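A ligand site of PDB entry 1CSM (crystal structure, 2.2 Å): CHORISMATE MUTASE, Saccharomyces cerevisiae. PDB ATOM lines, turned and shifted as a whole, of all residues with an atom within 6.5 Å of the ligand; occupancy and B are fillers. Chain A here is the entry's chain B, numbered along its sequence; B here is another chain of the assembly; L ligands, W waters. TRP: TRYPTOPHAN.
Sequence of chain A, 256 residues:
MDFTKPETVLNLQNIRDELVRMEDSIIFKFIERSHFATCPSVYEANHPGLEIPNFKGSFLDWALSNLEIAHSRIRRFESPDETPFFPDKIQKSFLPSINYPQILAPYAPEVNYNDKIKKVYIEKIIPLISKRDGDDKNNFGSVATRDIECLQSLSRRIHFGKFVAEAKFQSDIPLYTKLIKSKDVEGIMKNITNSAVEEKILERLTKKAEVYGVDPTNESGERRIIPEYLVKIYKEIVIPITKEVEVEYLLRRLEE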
ATOM      1  N   PHE A  36      26.823  10.477   1.030  1.00  0.00           N
ATOM      2  CA  PHE A  36      26.783  11.851   1.480  1.00  0.00           C
ATOM      3  C   PHE A  36      27.984  12.312   2.265  1.00  0.00           C
ATOM      4  O   PHE A  36      28.691  11.518   2.860  1.00  0.00           O
ATOM      5  CB  PHE A  36      25.552  12.069   2.349  1.00  0.00           C
ATOM      6  CG  PHE A  36      24.312  11.552   1.743  1.00  0.00           C
ATOM      7  CD1 PHE A  36      23.955  10.223   1.910  1.00  0.00           C
ATOM      8  CD2 PHE A  36      23.493  12.375   0.994  1.00  0.00           C
ATOM      9  CE1 PHE A  36      22.799   9.741   1.326  1.00  0.00           C
ATOM     10  CE2 PHE A  36      22.348  11.899   0.413  1.00  0.00           C
ATOM     11  CZ  PHE A  36      21.998  10.569   0.587  1.00  0.00           C
ATOM     12  N   PHE A  59      19.706  17.845  15.069  1.00  0.00           N
ATOM     13  CA  PHE A  59      18.730  17.496  14.052  1.00  0.00           C
ATOM     14  C   PHE A  59      18.610  15.955  14.168  1.00  0.00           C
ATOM     15  O   PHE A  59      17.506  15.379  14.176  1.00  0.00           O
ATOM     16  CB  PHE A  59      19.314  17.931  12.685  1.00  0.00           C
ATOM     17  CG  PHE A  59      18.394  17.771  11.515  1.00  0.00           C
ATOM     18  CD1 PHE A  59      18.384  16.598  10.792  1.00  0.00           C
ATOM     19  CD2 PHE A  59      17.614  18.826  11.087  1.00  0.00           C
ATOM     20  CE1 PHE A  59      17.628  16.484   9.634  1.00  0.00           C
ATOM     21  CE2 PHE A  59      16.857  18.725   9.933  1.00  0.00           C
ATOM     22  CZ  PHE A  59      16.859  17.546   9.210  1.00  0.00           C
ATOM     23  N   LYS A 137      23.999  21.134   2.750  1.00  0.00           N
ATOM     24  CA  LYS A 137      22.737  21.602   3.247  1.00  0.00           C
ATOM     25  C   LYS A 137      21.474  21.187   2.526  1.00  0.00           C
ATOM     26  O   LYS A 137      20.376  21.498   2.975  1.00  0.00           O
ATOM     27  CB  LYS A 137      22.759  23.098   3.539  1.00  0.00           C
ATOM     28  CG  LYS A 137      21.688  23.461   4.580  1.00  0.00           C
ATOM     29  CD  LYS A 137      21.965  24.764   5.342  1.00  0.00           C
ATOM     30  CE  LYS A 137      21.049  24.866   6.590  1.00  0.00           C
ATOM     31  NZ  LYS A 137      19.588  24.667   6.307  1.00  0.00           N
ATOM     32  N   ASN A 138      21.600  20.493   1.419  1.00  0.00           N
ATOM     33  CA  ASN A 138      20.410  20.036   0.727  1.00  0.00           C
ATOM     34  C   ASN A 138      20.150  18.562   1.130  1.00  0.00           C
ATOM     35  O   ASN A 138      19.223  17.940   0.609  1.00  0.00           O
ATOM     36  CB  ASN A 138      20.584  20.096  -0.800  1.00  0.00           C
ATOM     37  CG  ASN A 138      21.089  21.440  -1.285  1.00  0.00           C
ATOM     38  OD1 ASN A 138      21.932  21.500  -2.182  1.00  0.00           O
ATOM     39  ND2 ASN A 138      20.582  22.511  -0.696  1.00  0.00           N
ATOM     40  N   ASN A 139      20.966  18.011   2.017  1.00  0.00           N
ATOM     41  CA  ASN A 139      20.792  16.621   2.418  1.00  0.00           C
ATOM     42  C   ASN A 139      20.885  16.298   3.867  1.00  0.00           C
ATOM     43  O   ASN A 139      21.274  15.195   4.230  1.00  0.00           O
ATOM     44  CB  ASN A 139      21.762  15.744   1.654  1.00  0.00           C
ATOM     45  CG  ASN A 139      21.374  15.620   0.217  1.00  0.00           C
ATOM     46  OD1 ASN A 139      20.186  15.607  -0.096  1.00  0.00           O
ATOM     47  ND2 ASN A 139      22.339  15.580  -0.669  1.00  0.00           N
ATOM     48  N   PHE A 140      20.491  17.225   4.719  1.00  0.00           N
ATOM     49  CA  PHE A 140      20.541  16.970   6.125  1.00  0.00           C
ATOM     50  C   PHE A 140      19.535  15.873   6.492  1.00  0.00           C
ATOM     51  O   PHE A 140      19.882  14.912   7.170  1.00  0.00           O
ATOM     52  CB  PHE A 140      20.290  18.254   6.917  1.00  0.00           C
ATOM     53  CG  PHE A 140      21.458  19.223   6.897  1.00  0.00           C
ATOM     54  CD1 PHE A 140      22.661  18.882   6.298  1.00  0.00           C
ATOM     55  CD2 PHE A 140      21.359  20.459   7.500  1.00  0.00           C
ATOM     56  CE1 PHE A 140      23.743  19.768   6.309  1.00  0.00           C
ATOM     57  CE2 PHE A 140      22.440  21.344   7.510  1.00  0.00           C
ATOM     58  CZ  PHE A 140      23.622  20.994   6.918  1.00  0.00           C
ATOM     59  N   GLY A 141      18.317  15.979   5.970  1.00  0.00           N
ATOM     60  CA  GLY A 141      17.296  14.999   6.275  1.00  0.00           C
ATOM     61  C   GLY A 141      17.659  13.640   5.703  1.00  0.00           C
ATOM     62  O   GLY A 141      17.493  12.630   6.388  1.00  0.00           O
ATOM     63  N   SER A 142      18.129  13.608   4.461  1.00  0.00           N
ATOM     64  CA  SER A 142      18.535  12.356   3.821  1.00  0.00           C
ATOM     65  C   SER A 142      19.659  11.731   4.614  1.00  0.00           C
ATOM     66  O   SER A 142      19.744  10.516   4.714  1.00  0.00           O
ATOM     67  CB  SER A 142      19.008  12.591   2.397  1.00  0.00           C
ATOM     68  OG  SER A 142      17.934  12.926   1.547  1.00  0.00           O
ATOM     69  N   VAL A 143      20.517  12.565   5.181  1.00  0.00           N
ATOM     70  CA  VAL A 143      21.649  12.102   6.000  1.00  0.00           C
ATOM     71  C   VAL A 143      21.162  11.580   7.376  1.00  0.00           C
ATOM     72  O   VAL A 143      21.597  10.530   7.820  1.00  0.00           O
ATOM     73  CB  VAL A 143      22.698  13.235   6.204  1.00  0.00           C
ATOM     74  CG1 VAL A 143      23.509  13.041   7.487  1.00  0.00           C
ATOM     75  CG2 VAL A 143      23.628  13.289   5.005  1.00  0.00           C
ATOM     76  N   ALA A 144      20.285  12.318   8.038  1.00  0.00           N
ATOM     77  CA  ALA A 144      19.783  11.900   9.349  1.00  0.00           C
ATOM     78  C   ALA A 144      19.065  10.548   9.275  1.00  0.00           C
ATOM     79  O   ALA A 144      19.238   9.698  10.149  1.00  0.00           O
ATOM     80  CB  ALA A 144      18.865  12.958   9.903  1.00  0.00           C
ATOM     81  N   THR A 145      18.286  10.336   8.209  1.00  0.00           N
ATOM     82  CA  THR A 145      17.583   9.082   8.066  1.00  0.00           C
ATOM     83  C   THR A 145      18.527   7.896   7.784  1.00  0.00           C
ATOM     84  O   THR A 145      18.291   6.803   8.273  1.00  0.00           O
ATOM     85  CB  THR A 145      16.405   9.185   7.054  1.00  0.00           C
ATOM     86  OG1 THR A 145      16.893   9.492   5.748  1.00  0.00           O
ATOM     87  CG2 THR A 145      15.455  10.301   7.462  1.00  0.00           C
ATOM     88  N   ALA B  70       6.210  13.545  10.128  1.00  0.00           N
ATOM     89  CA  ALA B  70       7.390  13.998  10.830  1.00  0.00           C
ATOM     90  C   ALA B  70       8.354  14.565   9.827  1.00  0.00           C
ATOM     91  O   ALA B  70       8.797  15.699   9.941  1.00  0.00           O
ATOM     92  CB  ALA B  70       8.016  12.870  11.571  1.00  0.00           C
ATOM     93  N   HIS B  71       8.652  13.786   8.813  1.00  0.00           N
ATOM     94  CA  HIS B  71       9.570  14.257   7.808  1.00  0.00           C
ATOM     95  C   HIS B  71       9.151  15.568   7.122  1.00  0.00           C
ATOM     96  O   HIS B  71      10.000  16.398   6.805  1.00  0.00           O
ATOM     97  CB  HIS B  71       9.799  13.151   6.782  1.00  0.00           C
ATOM     98  CG  HIS B  71      10.598  12.013   7.306  1.00  0.00           C
ATOM     99  ND1 HIS B  71      11.004  10.993   6.480  1.00  0.00           N
ATOM    100  CD2 HIS B  71      11.119  11.820   8.545  1.00  0.00           C
ATOM    101  CE1 HIS B  71      11.767  10.213   7.225  1.00  0.00           C
ATOM    102  NE2 HIS B  71      11.860  10.677   8.491  1.00  0.00           N
ATOM    103  N   SER B  72       7.853  15.764   6.914  1.00  0.00           N
ATOM    104  CA  SER B  72       7.379  16.976   6.235  1.00  0.00           C
ATOM    105  C   SER B  72       7.712  18.251   7.004  1.00  0.00           C
ATOM    106  O   SER B  72       7.966  19.302   6.397  1.00  0.00           O
ATOM    107  CB  SER B  72       5.883  16.889   5.910  1.00  0.00           C
ATOM    108  OG  SER B  72       5.066  16.965   7.075  1.00  0.00           O
ATOM    109  N   ILE B  74      10.315  18.633   8.713  1.00  0.00           N
ATOM    110  CA  ILE B  74      11.737  18.835   8.503  1.00  0.00           C
ATOM    111  C   ILE B  74      12.058  18.940   6.991  1.00  0.00           C
ATOM    112  O   ILE B  74      13.032  18.391   6.460  1.00  0.00           O
ATOM    113  CB  ILE B  74      12.677  17.865   9.358  1.00  0.00           C
ATOM    114  CG1 ILE B  74      12.464  16.387   9.054  1.00  0.00           C
ATOM    115  CG2 ILE B  74      12.412  18.078  10.835  1.00  0.00           C
ATOM    116  CD1 ILE B  74      13.587  15.528   9.646  1.00  0.00           C
ATOM    117  N   ARG B  75      11.152  19.623   6.289  1.00  0.00           N
ATOM    118  CA  ARG B  75      11.290  19.925   4.869  1.00  0.00           C
ATOM    119  C   ARG B  75      11.430  18.775   3.914  1.00  0.00           C
ATOM    120  O   ARG B  75      11.916  18.946   2.789  1.00  0.00           O
ATOM    121  CB  ARG B  75      12.467  20.878   4.658  1.00  0.00           C
ATOM    122  CG  ARG B  75      12.505  22.087   5.582  1.00  0.00           C
ATOM    123  CD  ARG B  75      13.777  22.878   5.337  1.00  0.00           C
ATOM    124  NE  ARG B  75      14.982  22.062   5.494  1.00  0.00           N
ATOM    125  CZ  ARG B  75      16.180  22.547   5.825  1.00  0.00           C
ATOM    126  NH1 ARG B  75      16.338  23.837   6.029  1.00  0.00           N
ATOM    127  NH2 ARG B  75      17.216  21.732   5.957  1.00  0.00           N
ATOM    128  N   ARG B  76      10.973  17.602   4.283  1.00  0.00           N
ATOM    129  CA  ARG B  76      11.140  16.500   3.369  1.00  0.00           C
ATOM    130  C   ARG B  76      10.520  16.733   1.993  1.00  0.00           C
ATOM    131  O   ARG B  76      11.194  16.618   0.958  1.00  0.00           O
ATOM    132  CB  ARG B  76      10.609  15.182   3.948  1.00  0.00           C
ATOM    133  CG  ARG B  76      10.952  14.048   3.016  1.00  0.00           C
ATOM    134  CD  ARG B  76      10.529  12.690   3.485  1.00  0.00           C
ATOM    135  NE  ARG B  76      10.919  11.712   2.463  1.00  0.00           N
ATOM    136  CZ  ARG B  76      11.703  10.679   2.698  1.00  0.00           C
ATOM    137  NH1 ARG B  76      12.177  10.458   3.923  1.00  0.00           N
ATOM    138  NH2 ARG B  76      12.027   9.859   1.708  1.00  0.00           N
ATOM    139  N   PHE B  77       9.263  17.164   1.955  1.00  0.00           N
ATOM    140  CA  PHE B  77       8.617  17.291   0.673  1.00  0.00           C
ATOM    141  C   PHE B  77       8.713  18.598  -0.094  1.00  0.00           C
ATOM    142  O   PHE B  77       7.984  18.812  -1.045  1.00  0.00           O
ATOM    143  CB  PHE B  77       7.201  16.722   0.751  1.00  0.00           C
ATOM    144  CG  PHE B  77       7.166  15.291   1.217  1.00  0.00           C
ATOM    145  CD1 PHE B  77       7.511  14.264   0.350  1.00  0.00           C
ATOM    146  CD2 PHE B  77       6.868  14.994   2.542  1.00  0.00           C
ATOM    147  CE1 PHE B  77       7.575  12.938   0.792  1.00  0.00           C
ATOM    148  CE2 PHE B  77       6.912  13.675   3.007  1.00  0.00           C
ATOM    149  CZ  PHE B  77       7.280  12.645   2.131  1.00  0.00           C
ATOM    150  N   GLU B  78       9.643  19.459   0.298  1.00  0.00           N
ATOM    151  CA  GLU B  78       9.879  20.712  -0.439  1.00  0.00           C
ATOM    152  C   GLU B  78      10.814  20.368  -1.597  1.00  0.00           C
ATOM    153  O   GLU B  78      10.855  21.080  -2.585  1.00  0.00           O
ATOM    154  CB  GLU B  78      10.598  21.749   0.397  1.00  0.00           C
ATOM    155  CG  GLU B  78       9.875  22.258   1.601  1.00  0.00           C
ATOM    156  CD  GLU B  78      10.692  23.325   2.308  1.00  0.00           C
ATOM    157  OE1 GLU B  78      11.899  23.488   1.965  1.00  0.00           O
ATOM    158  OE2 GLU B  78      10.127  24.001   3.200  1.00  0.00           O
ATOM    159  N   SER B  79      11.598  19.303  -1.413  1.00  0.00           N
ATOM    160  CA  SER B  79      12.551  18.876  -2.416  1.00  0.00           C
ATOM    161  C   SER B  79      11.825  18.334  -3.640  1.00  0.00           C
ATOM    162  O   SER B  79      10.853  17.590  -3.530  1.00  0.00           O
ATOM    163  CB  SER B  79      13.507  17.817  -1.836  1.00  0.00           C
ATOM    164  OG  SER B  79      14.620  17.575  -2.687  1.00  0.00           O
ATOM    165  N   ASP B  81      12.691  16.040  -5.659  1.00  0.00           N
ATOM    166  CA  ASP B  81      12.773  14.613  -5.869  1.00  0.00           C
ATOM    167  C   ASP B  81      12.027  13.768  -4.835  1.00  0.00           C
ATOM    168  O   ASP B  81      12.165  12.546  -4.837  1.00  0.00           O
ATOM    169  CB  ASP B  81      14.218  14.127  -6.017  1.00  0.00           C
ATOM    170  CG  ASP B  81      15.020  14.208  -4.723  1.00  0.00           C
ATOM    171  OD1 ASP B  81      14.743  15.053  -3.852  1.00  0.00           O
ATOM    172  OD2 ASP B  81      15.991  13.437  -4.601  1.00  0.00           O
ATOM    173  N   GLU B  82      11.209  14.410  -3.990  1.00  0.00           N
ATOM    174  CA  GLU B  82      10.476  13.677  -2.960  1.00  0.00           C
ATOM    175  C   GLU B  82       8.962  13.862  -3.101  1.00  0.00           C
ATOM    176  O   GLU B  82       8.457  14.978  -2.965  1.00  0.00           O
ATOM    177  CB  GLU B  82      10.921  14.091  -1.564  1.00  0.00           C
ATOM    178  CG  GLU B  82      12.397  13.822  -1.252  1.00  0.00           C
ATOM    179  CD  GLU B  82      12.722  12.368  -0.956  1.00  0.00           C
ATOM    180  OE1 GLU B  82      11.801  11.614  -0.576  1.00  0.00           O
ATOM    181  OE2 GLU B  82      13.913  11.979  -1.062  1.00  0.00           O
ATOM    182  N   ILE B  98      14.760  26.092   1.998  1.00  0.00           N
ATOM    183  CA  ILE B  98      15.862  26.063   1.056  1.00  0.00           C
ATOM    184  C   ILE B  98      15.142  26.540  -0.204  1.00  0.00           C
ATOM    185  O   ILE B  98      14.150  25.946  -0.589  1.00  0.00           O
ATOM    186  CB  ILE B  98      16.345  24.616   0.871  1.00  0.00           C
ATOM    187  CG1 ILE B  98      17.069  24.148   2.128  1.00  0.00           C
ATOM    188  CG2 ILE B  98      17.201  24.479  -0.335  1.00  0.00           C
ATOM    189  CD1 ILE B  98      17.402  22.665   2.141  1.00  0.00           C
ATOM    190  N   TYR B 100      14.614  26.305  -3.478  1.00  0.00           N
ATOM    191  CA  TYR B 100      14.950  25.477  -4.632  1.00  0.00           C
ATOM    192  C   TYR B 100      14.595  26.232  -5.927  1.00  0.00           C
ATOM    193  O   TYR B 100      13.568  26.917  -6.007  1.00  0.00           O
ATOM    194  CB  TYR B 100      14.206  24.136  -4.586  1.00  0.00           C
ATOM    195  CG  TYR B 100      14.787  23.104  -3.626  1.00  0.00           C
ATOM    196  CD1 TYR B 100      15.973  22.442  -3.921  1.00  0.00           C
ATOM    197  CD2 TYR B 100      14.121  22.782  -2.429  1.00  0.00           C
ATOM    198  CE1 TYR B 100      16.512  21.464  -3.037  1.00  0.00           C
ATOM    199  CE2 TYR B 100      14.648  21.798  -1.550  1.00  0.00           C
ATOM    200  CZ  TYR B 100      15.841  21.149  -1.863  1.00  0.00           C
ATOM    201  OH  TYR B 100      16.354  20.182  -1.024  1.00  0.00           O
HETATM  202  N   TRP L   1      17.135  15.342   0.518  1.00  0.00           N
HETATM  203  CA  TRP L   1      16.196  16.363   1.071  1.00  0.00           C
HETATM  204  C   TRP L   1      16.701  16.784   2.447  1.00  0.00           C
HETATM  205  O   TRP L   1      16.188  17.756   3.051  1.00  0.00           O
HETATM  206  CB  TRP L   1      14.787  15.792   1.185  1.00  0.00           C
HETATM  207  CG  TRP L   1      14.674  14.688   2.179  1.00  0.00           C
HETATM  208  CD1 TRP L   1      14.833  13.357   1.952  1.00  0.00           C
HETATM  209  CD2 TRP L   1      14.358  14.839   3.578  1.00  0.00           C
HETATM  210  NE1 TRP L   1      14.619  12.655   3.128  1.00  0.00           N
HETATM  211  CE2 TRP L   1      14.334  13.545   4.137  1.00  0.00           C
HETATM  212  CE3 TRP L   1      14.100  15.936   4.411  1.00  0.00           C
HETATM  213  CZ2 TRP L   1      14.056  13.326   5.473  1.00  0.00           C
HETATM  214  CZ3 TRP L   1      13.827  15.712   5.741  1.00  0.00           C
HETATM  215  CH2 TRP L   1      13.796  14.420   6.262  1.00  0.00           C
HETATM  216  OXT TRP L   1      17.607  16.087   2.923  1.00  0.00           O
HETATM  217  O   HOH W   1      15.588   9.635   2.875  1.00  0.00           O
HETATM  218  O   HOH W   2      18.629  19.491   3.895  1.00  0.00           O
HETATM  219  O   HOH W   3      15.842  18.964   5.638  1.00  0.00           O
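Water W3 lies within hydrogen-bond range of O of the ligand (2.9 Å), O of Ile 74 of chain B (3.0 Å) and NH2 of Arg 75 of chain B (3.1 Å). Water W1 lies within hydrogen-bond range of OG1 of Thr 145 and NE1 of the ligand.
NH1 of Arg 76 of chain B lies close to NE1 of the ligand, 3.4 Å away. Residues that only touch the ligand: Ile 74 of chain B (2.9 Å), Glu 82 of chain B (3.4 Å), Phe 140 (3.6 Å), Ser 79 of chain B (3.9 Å), Thr 145 (3.9 Å), Arg 75 of chain B (3.9 Å) and His 71 of chain B (3.97 Å). Hydrophobic or aromatic side chains that line the ligand: Ile 74 of chain B. 12 residues have an atom within 4 Å of the ligand: Asn 138, Asn 139, Phe 140, Gly 141, Ser 142, Thr 145, His 71 of chain B, Ile 74 of chain B, Arg 75 of chain B, Arg 76 of chain B, Ser 79 of chain B and Glu 82 of chain B. The nearest printed residue that does not touch the ligand is Tyr 100 of chain B (4.4 Å).
A nitrogen (N) of the ligand is in hydrogen-bond range of the side-chain hydroxyl (OG) of Ser 142, 2.7 Å away. N of Gly 141 is in hydrogen-bond range of OXT of the ligand (3.1 Å). O of Asn 138 lies close to N of the ligand, 3.3 Å away. N of Ser 142 sits at hydrogen-bond distance from OXT of the ligand, at 3.0 Å. A nitrogen (N) of the ligand is in hydrogen-bond range of the side-chain amide oxygen (OD1) of Asn 139, 3.1 Å away.
The backbone carbonyl oxygen of Ser 142 sits at hydrogen-bond distance from the side-chain hydroxyl of Thr 145, 3.2 Å away. The backbone carbonyl oxygen (O) of Gly 141 sits at hydrogen-bond distance from the side-chain hydroxyl (OG1) of Thr 145 (3.3 Å). NH2 of Arg 76 of chain B is in salt-bridge range of OE1 of Glu 82 of chain B (2.9 Å). The side-chain carboxylate (OD1) of Asp 81 of chain B is in hydrogen-bond range of the side-chain hydroxyl (OG) of Ser 79 of chain B (2.8 Å). A ring nitrogen (ND1) of His 71 of chain B is in hydrogen-bond range of the guanidinium group (NH1) of Arg 76 of chain B (2.9 Å).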
